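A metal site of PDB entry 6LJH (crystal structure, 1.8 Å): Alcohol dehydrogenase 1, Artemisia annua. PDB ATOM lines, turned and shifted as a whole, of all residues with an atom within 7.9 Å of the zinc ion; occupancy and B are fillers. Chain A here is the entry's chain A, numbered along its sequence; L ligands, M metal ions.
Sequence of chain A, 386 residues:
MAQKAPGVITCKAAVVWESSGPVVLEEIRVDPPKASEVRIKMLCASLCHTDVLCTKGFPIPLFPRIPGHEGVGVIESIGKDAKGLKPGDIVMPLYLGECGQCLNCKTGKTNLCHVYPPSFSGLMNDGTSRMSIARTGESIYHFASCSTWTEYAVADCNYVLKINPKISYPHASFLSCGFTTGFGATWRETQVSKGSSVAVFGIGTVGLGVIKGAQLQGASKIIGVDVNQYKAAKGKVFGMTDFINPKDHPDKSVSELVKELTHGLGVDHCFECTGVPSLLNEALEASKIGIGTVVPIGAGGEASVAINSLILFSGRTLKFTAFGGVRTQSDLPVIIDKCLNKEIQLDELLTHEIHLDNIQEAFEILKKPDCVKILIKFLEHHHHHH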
ATOM      1  N   SER A  46      -4.720  31.990  -2.700  1.00  0.00           N
ATOM      2  CA  SER A  46      -4.449  31.482  -4.036  1.00  0.00           C
ATOM      3  C   SER A  46      -5.279  30.216  -4.252  1.00  0.00           C
ATOM      4  O   SER A  46      -6.226  29.927  -3.508  1.00  0.00           O
ATOM      5  CB  SER A  46      -2.934  31.281  -4.245  1.00  0.00           C
ATOM      6  OG  SER A  46      -2.656  30.970  -5.597  1.00  0.00           O
ATOM      7  N   LEU A  47      -4.920  29.460  -5.294  1.00  0.00           N
ATOM      8  CA  LEU A  47      -5.730  28.371  -5.819  1.00  0.00           C
ATOM      9  C   LEU A  47      -4.792  27.359  -6.443  1.00  0.00           C
ATOM     10  O   LEU A  47      -3.821  27.733  -7.113  1.00  0.00           O
ATOM     11  CB  LEU A  47      -6.719  28.889  -6.881  1.00  0.00           C
ATOM     12  CG  LEU A  47      -7.616  27.974  -7.721  1.00  0.00           C
ATOM     13  CD1 LEU A  47      -8.814  28.772  -8.243  1.00  0.00           C
ATOM     14  CD2 LEU A  47      -6.884  27.332  -8.898  1.00  0.00           C
ATOM     15  N   CYS A  48      -5.080  26.079  -6.248  1.00  0.00           N
ATOM     16  CA  CYS A  48      -4.429  25.031  -7.020  1.00  0.00           C
ATOM     17  C   CYS A  48      -5.459  23.955  -7.348  1.00  0.00           C
ATOM     18  O   CYS A  48      -6.648  24.083  -7.033  1.00  0.00           O
ATOM     19  CB  CYS A  48      -3.207  24.457  -6.288  1.00  0.00           C
ATOM     20  SG  CYS A  48      -3.568  23.228  -5.021  1.00  0.00           S
ATOM     21  N   HIS A  49      -5.001  22.885  -8.023  1.00  0.00           N
ATOM     22  CA  HIS A  49      -5.926  21.859  -8.517  1.00  0.00           C
ATOM     23  C   HIS A  49      -6.718  21.222  -7.381  1.00  0.00           C
ATOM     24  O   HIS A  49      -7.868  20.794  -7.586  1.00  0.00           O
ATOM     25  CB  HIS A  49      -5.141  20.793  -9.278  1.00  0.00           C
ATOM     26  CG  HIS A  49      -6.016  19.734  -9.871  1.00  0.00           C
ATOM     27  ND1 HIS A  49      -6.905  19.986 -10.893  1.00  0.00           N
ATOM     28  CD2 HIS A  49      -6.142  18.408  -9.578  1.00  0.00           C
ATOM     29  CE1 HIS A  49      -7.534  18.869 -11.207  1.00  0.00           C
ATOM     30  NE2 HIS A  49      -7.090  17.899 -10.431  1.00  0.00           N
ATOM     31  N   THR A  50      -6.134  21.150  -6.189  1.00  0.00           N
ATOM     32  CA  THR A  50      -6.828  20.558  -5.055  1.00  0.00           C
ATOM     33  C   THR A  50      -8.123  21.312  -4.740  1.00  0.00           C
ATOM     34  O   THR A  50      -9.109  20.705  -4.328  1.00  0.00           O
ATOM     35  CB  THR A  50      -5.881  20.531  -3.854  1.00  0.00           C
ATOM     36  OG1 THR A  50      -4.720  19.767  -4.204  1.00  0.00           O
ATOM     37  CG2 THR A  50      -6.551  19.921  -2.632  1.00  0.00           C
ATOM     38  N   ASP A  51      -8.141  22.634  -4.962  1.00  0.00           N
ATOM     39  CA  ASP A  51      -9.378  23.394  -4.759  1.00  0.00           C
ATOM     40  C   ASP A  51     -10.402  23.066  -5.834  1.00  0.00           C
ATOM     41  O   ASP A  51     -11.606  22.991  -5.545  1.00  0.00           O
ATOM     42  CB  ASP A  51      -9.074  24.889  -4.765  1.00  0.00           C
ATOM     43  CG  ASP A  51      -8.124  25.291  -3.671  1.00  0.00           C
ATOM     44  OD1 ASP A  51      -8.412  24.951  -2.508  1.00  0.00           O
ATOM     45  OD2 ASP A  51      -7.087  25.919  -3.963  1.00  0.00           O
ATOM     46  N   GLY A  68     -10.405  26.687  -0.689  1.00  0.00           N
ATOM     47  CA  GLY A  68      -9.217  27.484  -0.444  1.00  0.00           C
ATOM     48  C   GLY A  68      -8.381  26.954   0.705  1.00  0.00           C
ATOM     49  O   GLY A  68      -8.857  26.829   1.821  1.00  0.00           O
ATOM     50  N   HIS A  69      -7.129  26.612   0.421  1.00  0.00           N
ATOM     51  CA  HIS A  69      -6.177  26.230   1.452  1.00  0.00           C
ATOM     52  C   HIS A  69      -4.917  27.086   1.423  1.00  0.00           C
ATOM     53  O   HIS A  69      -4.167  27.069   2.409  1.00  0.00           O
ATOM     54  CB  HIS A  69      -5.781  24.752   1.287  1.00  0.00           C
ATOM     55  CG  HIS A  69      -5.221  24.449  -0.064  1.00  0.00           C
ATOM     56  ND1 HIS A  69      -6.001  24.406  -1.201  1.00  0.00           N
ATOM     57  CD2 HIS A  69      -3.944  24.223  -0.464  1.00  0.00           C
ATOM     58  CE1 HIS A  69      -5.226  24.162  -2.248  1.00  0.00           C
ATOM     59  NE2 HIS A  69      -3.977  24.050  -1.826  1.00  0.00           N
ATOM     60  N   GLU A  70      -4.657  27.792   0.327  1.00  0.00           N
ATOM     61  CA  GLU A  70      -3.464  28.609   0.175  1.00  0.00           C
ATOM     62  C   GLU A  70      -3.781  30.052   0.521  1.00  0.00           C
ATOM     63  O   GLU A  70      -4.749  30.626   0.026  1.00  0.00           O
ATOM     64  CB  GLU A  70      -2.945  28.544  -1.271  1.00  0.00           C
ATOM     65  CG  GLU A  70      -2.717  27.137  -1.766  1.00  0.00           C
ATOM     66  CD  GLU A  70      -2.174  27.088  -3.181  1.00  0.00           C
ATOM     67  OE1 GLU A  70      -1.969  28.167  -3.774  1.00  0.00           O
ATOM     68  OE2 GLU A  70      -1.975  25.964  -3.697  1.00  0.00           O
ATOM     69  N   PHE A 143     -12.270  23.993   4.326  1.00  0.00           N
ATOM     70  CA  PHE A 143     -11.388  23.186   3.514  1.00  0.00           C
ATOM     71  C   PHE A 143     -10.065  22.952   4.244  1.00  0.00           C
ATOM     72  O   PHE A 143      -9.484  23.877   4.821  1.00  0.00           O
ATOM     73  CB  PHE A 143     -11.112  23.839   2.173  1.00  0.00           C
ATOM     74  CG  PHE A 143     -10.423  22.927   1.216  1.00  0.00           C
ATOM     75  CD1 PHE A 143     -11.082  21.831   0.691  1.00  0.00           C
ATOM     76  CD2 PHE A 143      -9.085  23.101   0.918  1.00  0.00           C
ATOM     77  CE1 PHE A 143     -10.443  20.953  -0.168  1.00  0.00           C
ATOM     78  CE2 PHE A 143      -8.434  22.230   0.057  1.00  0.00           C
ATOM     79  CZ  PHE A 143      -9.125  21.156  -0.487  1.00  0.00           C
ATOM     80  N   SER A 173       1.668  33.244   0.336  1.00  0.00           N
ATOM     81  CA  SER A 173       0.578  32.415  -0.176  1.00  0.00           C
ATOM     82  C   SER A 173       1.100  31.284  -1.051  1.00  0.00           C
ATOM     83  O   SER A 173       0.649  30.136  -0.939  1.00  0.00           O
ATOM     84  CB  SER A 173      -0.417  33.277  -0.965  1.00  0.00           C
ATOM     85  OG  SER A 173      -1.044  34.219  -0.120  1.00  0.00           O
ATOM     86  N   PHE A 174       2.053  31.593  -1.928  1.00  0.00           N
ATOM     87  CA  PHE A 174       2.567  30.538  -2.810  1.00  0.00           C
ATOM     88  C   PHE A 174       3.396  29.521  -2.029  1.00  0.00           C
ATOM     89  O   PHE A 174       3.413  28.334  -2.387  1.00  0.00           O
ATOM     90  CB  PHE A 174       3.395  31.136  -3.945  1.00  0.00           C
ATOM     91  CG  PHE A 174       2.641  32.142  -4.777  1.00  0.00           C
ATOM     92  CD1 PHE A 174       1.258  32.103  -4.839  1.00  0.00           C
ATOM     93  CD2 PHE A 174       3.318  33.107  -5.485  1.00  0.00           C
ATOM     94  CE1 PHE A 174       0.556  33.028  -5.597  1.00  0.00           C
ATOM     95  CE2 PHE A 174       2.624  34.034  -6.237  1.00  0.00           C
ATOM     96  CZ  PHE A 174       1.250  33.998  -6.295  1.00  0.00           C
ATOM     97  N   SER A 176       2.737  28.480   0.911  1.00  0.00           N
ATOM     98  CA  SER A 176       1.910  27.602   1.728  1.00  0.00           C
ATOM     99  C   SER A 176       1.561  26.283   1.030  1.00  0.00           C
ATOM    100  O   SER A 176       0.962  25.423   1.680  1.00  0.00           O
ATOM    101  CB  SER A 176       0.642  28.330   2.166  1.00  0.00           C
ATOM    102  OG  SER A 176      -0.267  28.471   1.096  1.00  0.00           O
ATOM    103  N   CYS A 177       1.936  26.078  -0.238  1.00  0.00           N
ATOM    104  CA  CYS A 177       1.582  24.816  -0.900  1.00  0.00           C
ATOM    105  C   CYS A 177       2.620  24.368  -1.943  1.00  0.00           C
ATOM    106  O   CYS A 177       3.664  23.823  -1.579  1.00  0.00           O
ATOM    107  CB  CYS A 177       0.190  24.910  -1.548  1.00  0.00           C
ATOM    108  SG  CYS A 177      -0.451  23.337  -2.278  1.00  0.00           S
ATOM    109  N   GLY A 178       2.351  24.628  -3.218  1.00  0.00           N
ATOM    110  CA  GLY A 178       3.020  23.876  -4.282  1.00  0.00           C
ATOM    111  C   GLY A 178       4.522  24.133  -4.399  1.00  0.00           C
ATOM    112  O   GLY A 178       5.310  23.191  -4.523  1.00  0.00           O
ATOM    113  N   PHE A 179       4.931  25.400  -4.430  1.00  0.00           N
ATOM    114  CA  PHE A 179       6.353  25.661  -4.634  1.00  0.00           C
ATOM    115  C   PHE A 179       7.166  25.058  -3.506  1.00  0.00           C
ATOM    116  O   PHE A 179       8.218  24.445  -3.748  1.00  0.00           O
ATOM    117  CB  PHE A 179       6.614  27.170  -4.751  1.00  0.00           C
ATOM    118  CG  PHE A 179       8.046  27.498  -5.137  1.00  0.00           C
ATOM    119  CD1 PHE A 179       9.023  27.654  -4.152  1.00  0.00           C
ATOM    120  CD2 PHE A 179       8.403  27.658  -6.467  1.00  0.00           C
ATOM    121  CE1 PHE A 179      10.337  27.962  -4.498  1.00  0.00           C
ATOM    122  CE2 PHE A 179       9.708  27.975  -6.825  1.00  0.00           C
ATOM    123  CZ  PHE A 179      10.673  28.126  -5.836  1.00  0.00           C
ATOM    124  N   THR A 181       6.365  22.457  -1.631  1.00  0.00           N
ATOM    125  CA  THR A 181       6.340  21.015  -1.834  1.00  0.00           C
ATOM    126  C   THR A 181       7.443  20.579  -2.792  1.00  0.00           C
ATOM    127  O   THR A 181       8.228  19.676  -2.477  1.00  0.00           O
ATOM    128  CB  THR A 181       4.958  20.602  -2.355  1.00  0.00           C
ATOM    129  OG1 THR A 181       3.983  20.813  -1.327  1.00  0.00           O
ATOM    130  CG2 THR A 181       4.965  19.149  -2.753  1.00  0.00           C
ATOM    131  N   THR A 205       3.905  25.398 -10.489  1.00  0.00           N
ATOM    132  CA  THR A 205       4.575  25.883  -9.293  1.00  0.00           C
ATOM    133  C   THR A 205       5.353  24.758  -8.588  1.00  0.00           C
ATOM    134  O   THR A 205       6.459  24.996  -8.068  1.00  0.00           O
ATOM    135  CB  THR A 205       3.570  26.549  -8.352  1.00  0.00           C
ATOM    136  OG1 THR A 205       4.277  27.202  -7.279  1.00  0.00           O
ATOM    137  CG2 THR A 205       2.580  25.518  -7.759  1.00  0.00           C
ATOM    138  N   VAL A 206       4.822  23.532  -8.599  1.00  0.00           N
ATOM    139  CA  VAL A 206       5.531  22.412  -7.962  1.00  0.00           C
ATOM    140  C   VAL A 206       6.846  22.136  -8.680  1.00  0.00           C
ATOM    141  O   VAL A 206       7.907  22.072  -8.053  1.00  0.00           O
ATOM    142  CB  VAL A 206       4.657  21.149  -7.922  1.00  0.00           C
ATOM    143  CG1 VAL A 206       5.474  19.970  -7.402  1.00  0.00           C
ATOM    144  CG2 VAL A 206       3.419  21.375  -7.068  1.00  0.00           C
ATOM    145  N   PHE A 323       3.463  17.051   1.121  1.00  0.00           N
ATOM    146  CA  PHE A 323       4.011  18.387   1.335  1.00  0.00           C
ATOM    147  C   PHE A 323       5.523  18.387   1.180  1.00  0.00           C
ATOM    148  O   PHE A 323       6.260  19.076   1.886  1.00  0.00           O
ATOM    149  CB  PHE A 323       3.579  18.949   2.699  1.00  0.00           C
ATOM    150  CG  PHE A 323       3.674  20.450   2.784  1.00  0.00           C
ATOM    151  CD1 PHE A 323       2.954  21.257   1.904  1.00  0.00           C
ATOM    152  CD2 PHE A 323       4.473  21.046   3.746  1.00  0.00           C
ATOM    153  CE1 PHE A 323       3.042  22.643   1.982  1.00  0.00           C
ATOM    154  CE2 PHE A 323       4.577  22.425   3.840  1.00  0.00           C
ATOM    155  CZ  PHE A 323       3.857  23.245   2.954  1.00  0.00           C
ATOM    156  N   LYS A 373       0.478  31.103 -11.321  1.00  0.00           N
ATOM    157  CA  LYS A 373      -0.243  31.223 -10.049  1.00  0.00           C
ATOM    158  C   LYS A 373      -1.209  32.404 -10.112  1.00  0.00           C
ATOM    159  O   LYS A 373      -0.862  33.457 -10.645  1.00  0.00           O
ATOM    160  CB  LYS A 373       0.715  31.405  -8.856  1.00  0.00           C
ATOM    161  CG  LYS A 373       1.506  30.147  -8.446  1.00  0.00           C
ATOM    162  CD  LYS A 373       0.594  28.959  -8.101  1.00  0.00           C
ATOM    163  CE  LYS A 373      -0.137  29.161  -6.761  1.00  0.00           C
ATOM    164  NZ  LYS A 373      -0.994  27.986  -6.467  1.00  0.00           N
HETATM  165  P1  LIG L   1       0.101  22.913 -12.573  1.00  0.00           P
HETATM  166  O1  LIG L   1       0.366  24.391 -12.377  1.00  0.00           O
HETATM  167  O2  LIG L   1      -1.201  22.601 -13.286  1.00  0.00           O
HETATM  168  O3  LIG L   1       1.330  22.237 -13.394  1.00  0.00           O
HETATM  169  C1  LIG L   1       1.082  21.049 -14.066  1.00  0.00           C
HETATM  170  C2  LIG L   1       1.952  21.168 -15.289  1.00  0.00           C
HETATM  171  O4  LIG L   1       2.055  19.715 -15.892  1.00  0.00           O
HETATM  172  C3  LIG L   1       1.432  22.016 -16.231  1.00  0.00           C
HETATM  173  O5  LIG L   1       2.474  22.976 -16.697  1.00  0.00           O
HETATM  174  C4  LIG L   1       1.010  21.121 -17.390  1.00  0.00           C
HETATM  175  O6  LIG L   1       1.211  21.704 -18.619  1.00  0.00           O
HETATM  176  C5  LIG L   1       1.979  19.890 -17.192  1.00  0.00           C
HETATM  177  N1  LIG L   1       1.386  18.697 -17.751  1.00  0.00           N
HETATM  178  C6  LIG L   1       0.122  18.256 -17.621  1.00  0.00           C
HETATM  179  N2  LIG L   1       0.017  17.084 -18.311  1.00  0.00           N
HETATM  180  C7  LIG L   1       1.222  16.827 -18.834  1.00  0.00           C
HETATM  181  C8  LIG L   1       1.756  15.697 -19.690  1.00  0.00           C
HETATM  182  N3  LIG L   1       0.879  14.615 -20.077  1.00  0.00           N
HETATM  183  N4  LIG L   1       3.109  15.706 -20.078  1.00  0.00           N
HETATM  184  C9  LIG L   1       4.003  16.753 -19.699  1.00  0.00           C
HETATM  185  N5  LIG L   1       3.490  17.848 -18.896  1.00  0.00           N
HETATM  186  C10 LIG L   1       2.068  17.833 -18.473  1.00  0.00           C
HETATM  187  O7  LIG L   1      -0.044  22.096 -11.180  1.00  0.00           O
HETATM  188  P2  LIG L   1       0.851  22.271  -9.829  1.00  0.00           P
HETATM  189  O8  LIG L   1       0.272  23.295  -8.947  1.00  0.00           O
HETATM  190  O9  LIG L   1       2.245  22.613 -10.107  1.00  0.00           O
HETATM  191  O10 LIG L   1       0.720  20.800  -9.134  1.00  0.00           O
HETATM  192  C11 LIG L   1       1.265  19.744  -9.891  1.00  0.00           C
HETATM  193  C12 LIG L   1       0.342  18.571  -9.955  1.00  0.00           C
HETATM  194  O11 LIG L   1       0.154  18.019  -8.476  1.00  0.00           O
HETATM  195  C13 LIG L   1      -0.906  18.851 -10.422  1.00  0.00           C
HETATM  196  O12 LIG L   1      -0.974  18.553 -11.858  1.00  0.00           O
HETATM  197  C14 LIG L   1      -1.826  17.943  -9.617  1.00  0.00           C
HETATM  198  O13 LIG L   1      -1.840  16.678 -10.098  1.00  0.00           O
HETATM  199  C15 LIG L   1      -1.102  17.797  -8.244  1.00  0.00           C
HETATM  200  N6  LIG L   1      -1.248  18.875  -7.348  1.00  0.00           N
HETATM  201  C16 LIG L   1      -0.296  18.833  -6.223  1.00  0.00           C
HETATM  202  C17 LIG L   1      -0.277  19.938  -5.196  1.00  0.00           C
HETATM  203  C18 LIG L   1       0.692  19.830  -4.045  1.00  0.00           C
HETATM  204  O14 LIG L   1       0.756  20.673  -3.221  1.00  0.00           O
HETATM  205  N7  LIG L   1       1.524  18.655  -3.986  1.00  0.00           N
HETATM  206  C19 LIG L   1      -1.229  21.065  -5.349  1.00  0.00           C
HETATM  207  C20 LIG L   1      -2.160  21.072  -6.527  1.00  0.00           C
HETATM  208  C21 LIG L   1      -2.195  19.975  -7.571  1.00  0.00           C
HETATM  209 ZN    ZN M   1      -2.456  24.076  -3.185  1.00  0.00          ZN
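SG of Cys 177 sits close to O14 of the ligand (3.1 Å). The backbone NH (N) of Thr 205 lies within hydrogen-bond range of an oxygen (O9) of the ligand. O9 of the ligand is in hydrogen-bond range of N of Val 206 (3.1 Å).
OE1 of Glu 70 lies within salt-bridge range of NZ of Lys 373, 2.9 Å away. The backbone carbonyl oxygen (O) of Glu 70 lies within hydrogen-bond range of the backbone NH (N) of Ser 46 (3.0 Å). The side-chain carboxylate (OD1) of Asp 51 sits at hydrogen-bond distance from a ring nitrogen (ND1) of His 69, 2.8 Å away. The side-chain sulfur (SG) of Cys 48 sits close to the backbone NH (N) of Thr 50. The backbone NH (N) of Cys 48 is in hydrogen-bond range of the side-chain carboxylate (OD2) of Asp 51 (3.0 Å). OG1 of Thr 181 lies within hydrogen-bond range of O of Cys 177 (3.0 Å).
Four residues have an atom within 4 Å of the zinc ion: Cys 48, His 69, Glu 70 and Cys 177.
The zinc ion is bound by OE2 of Glu 70 (2.0 Å). The zinc ion is bound by NE2 of His 69. The zinc ion is bound by the side-chain sulfur (SG) of Cys 48 (2.3 Å). The side-chain sulfur (SG) of Cys 177 is bound to the zinc ion (2.3 Å). The zinc ion has four donor atoms within binding distance.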
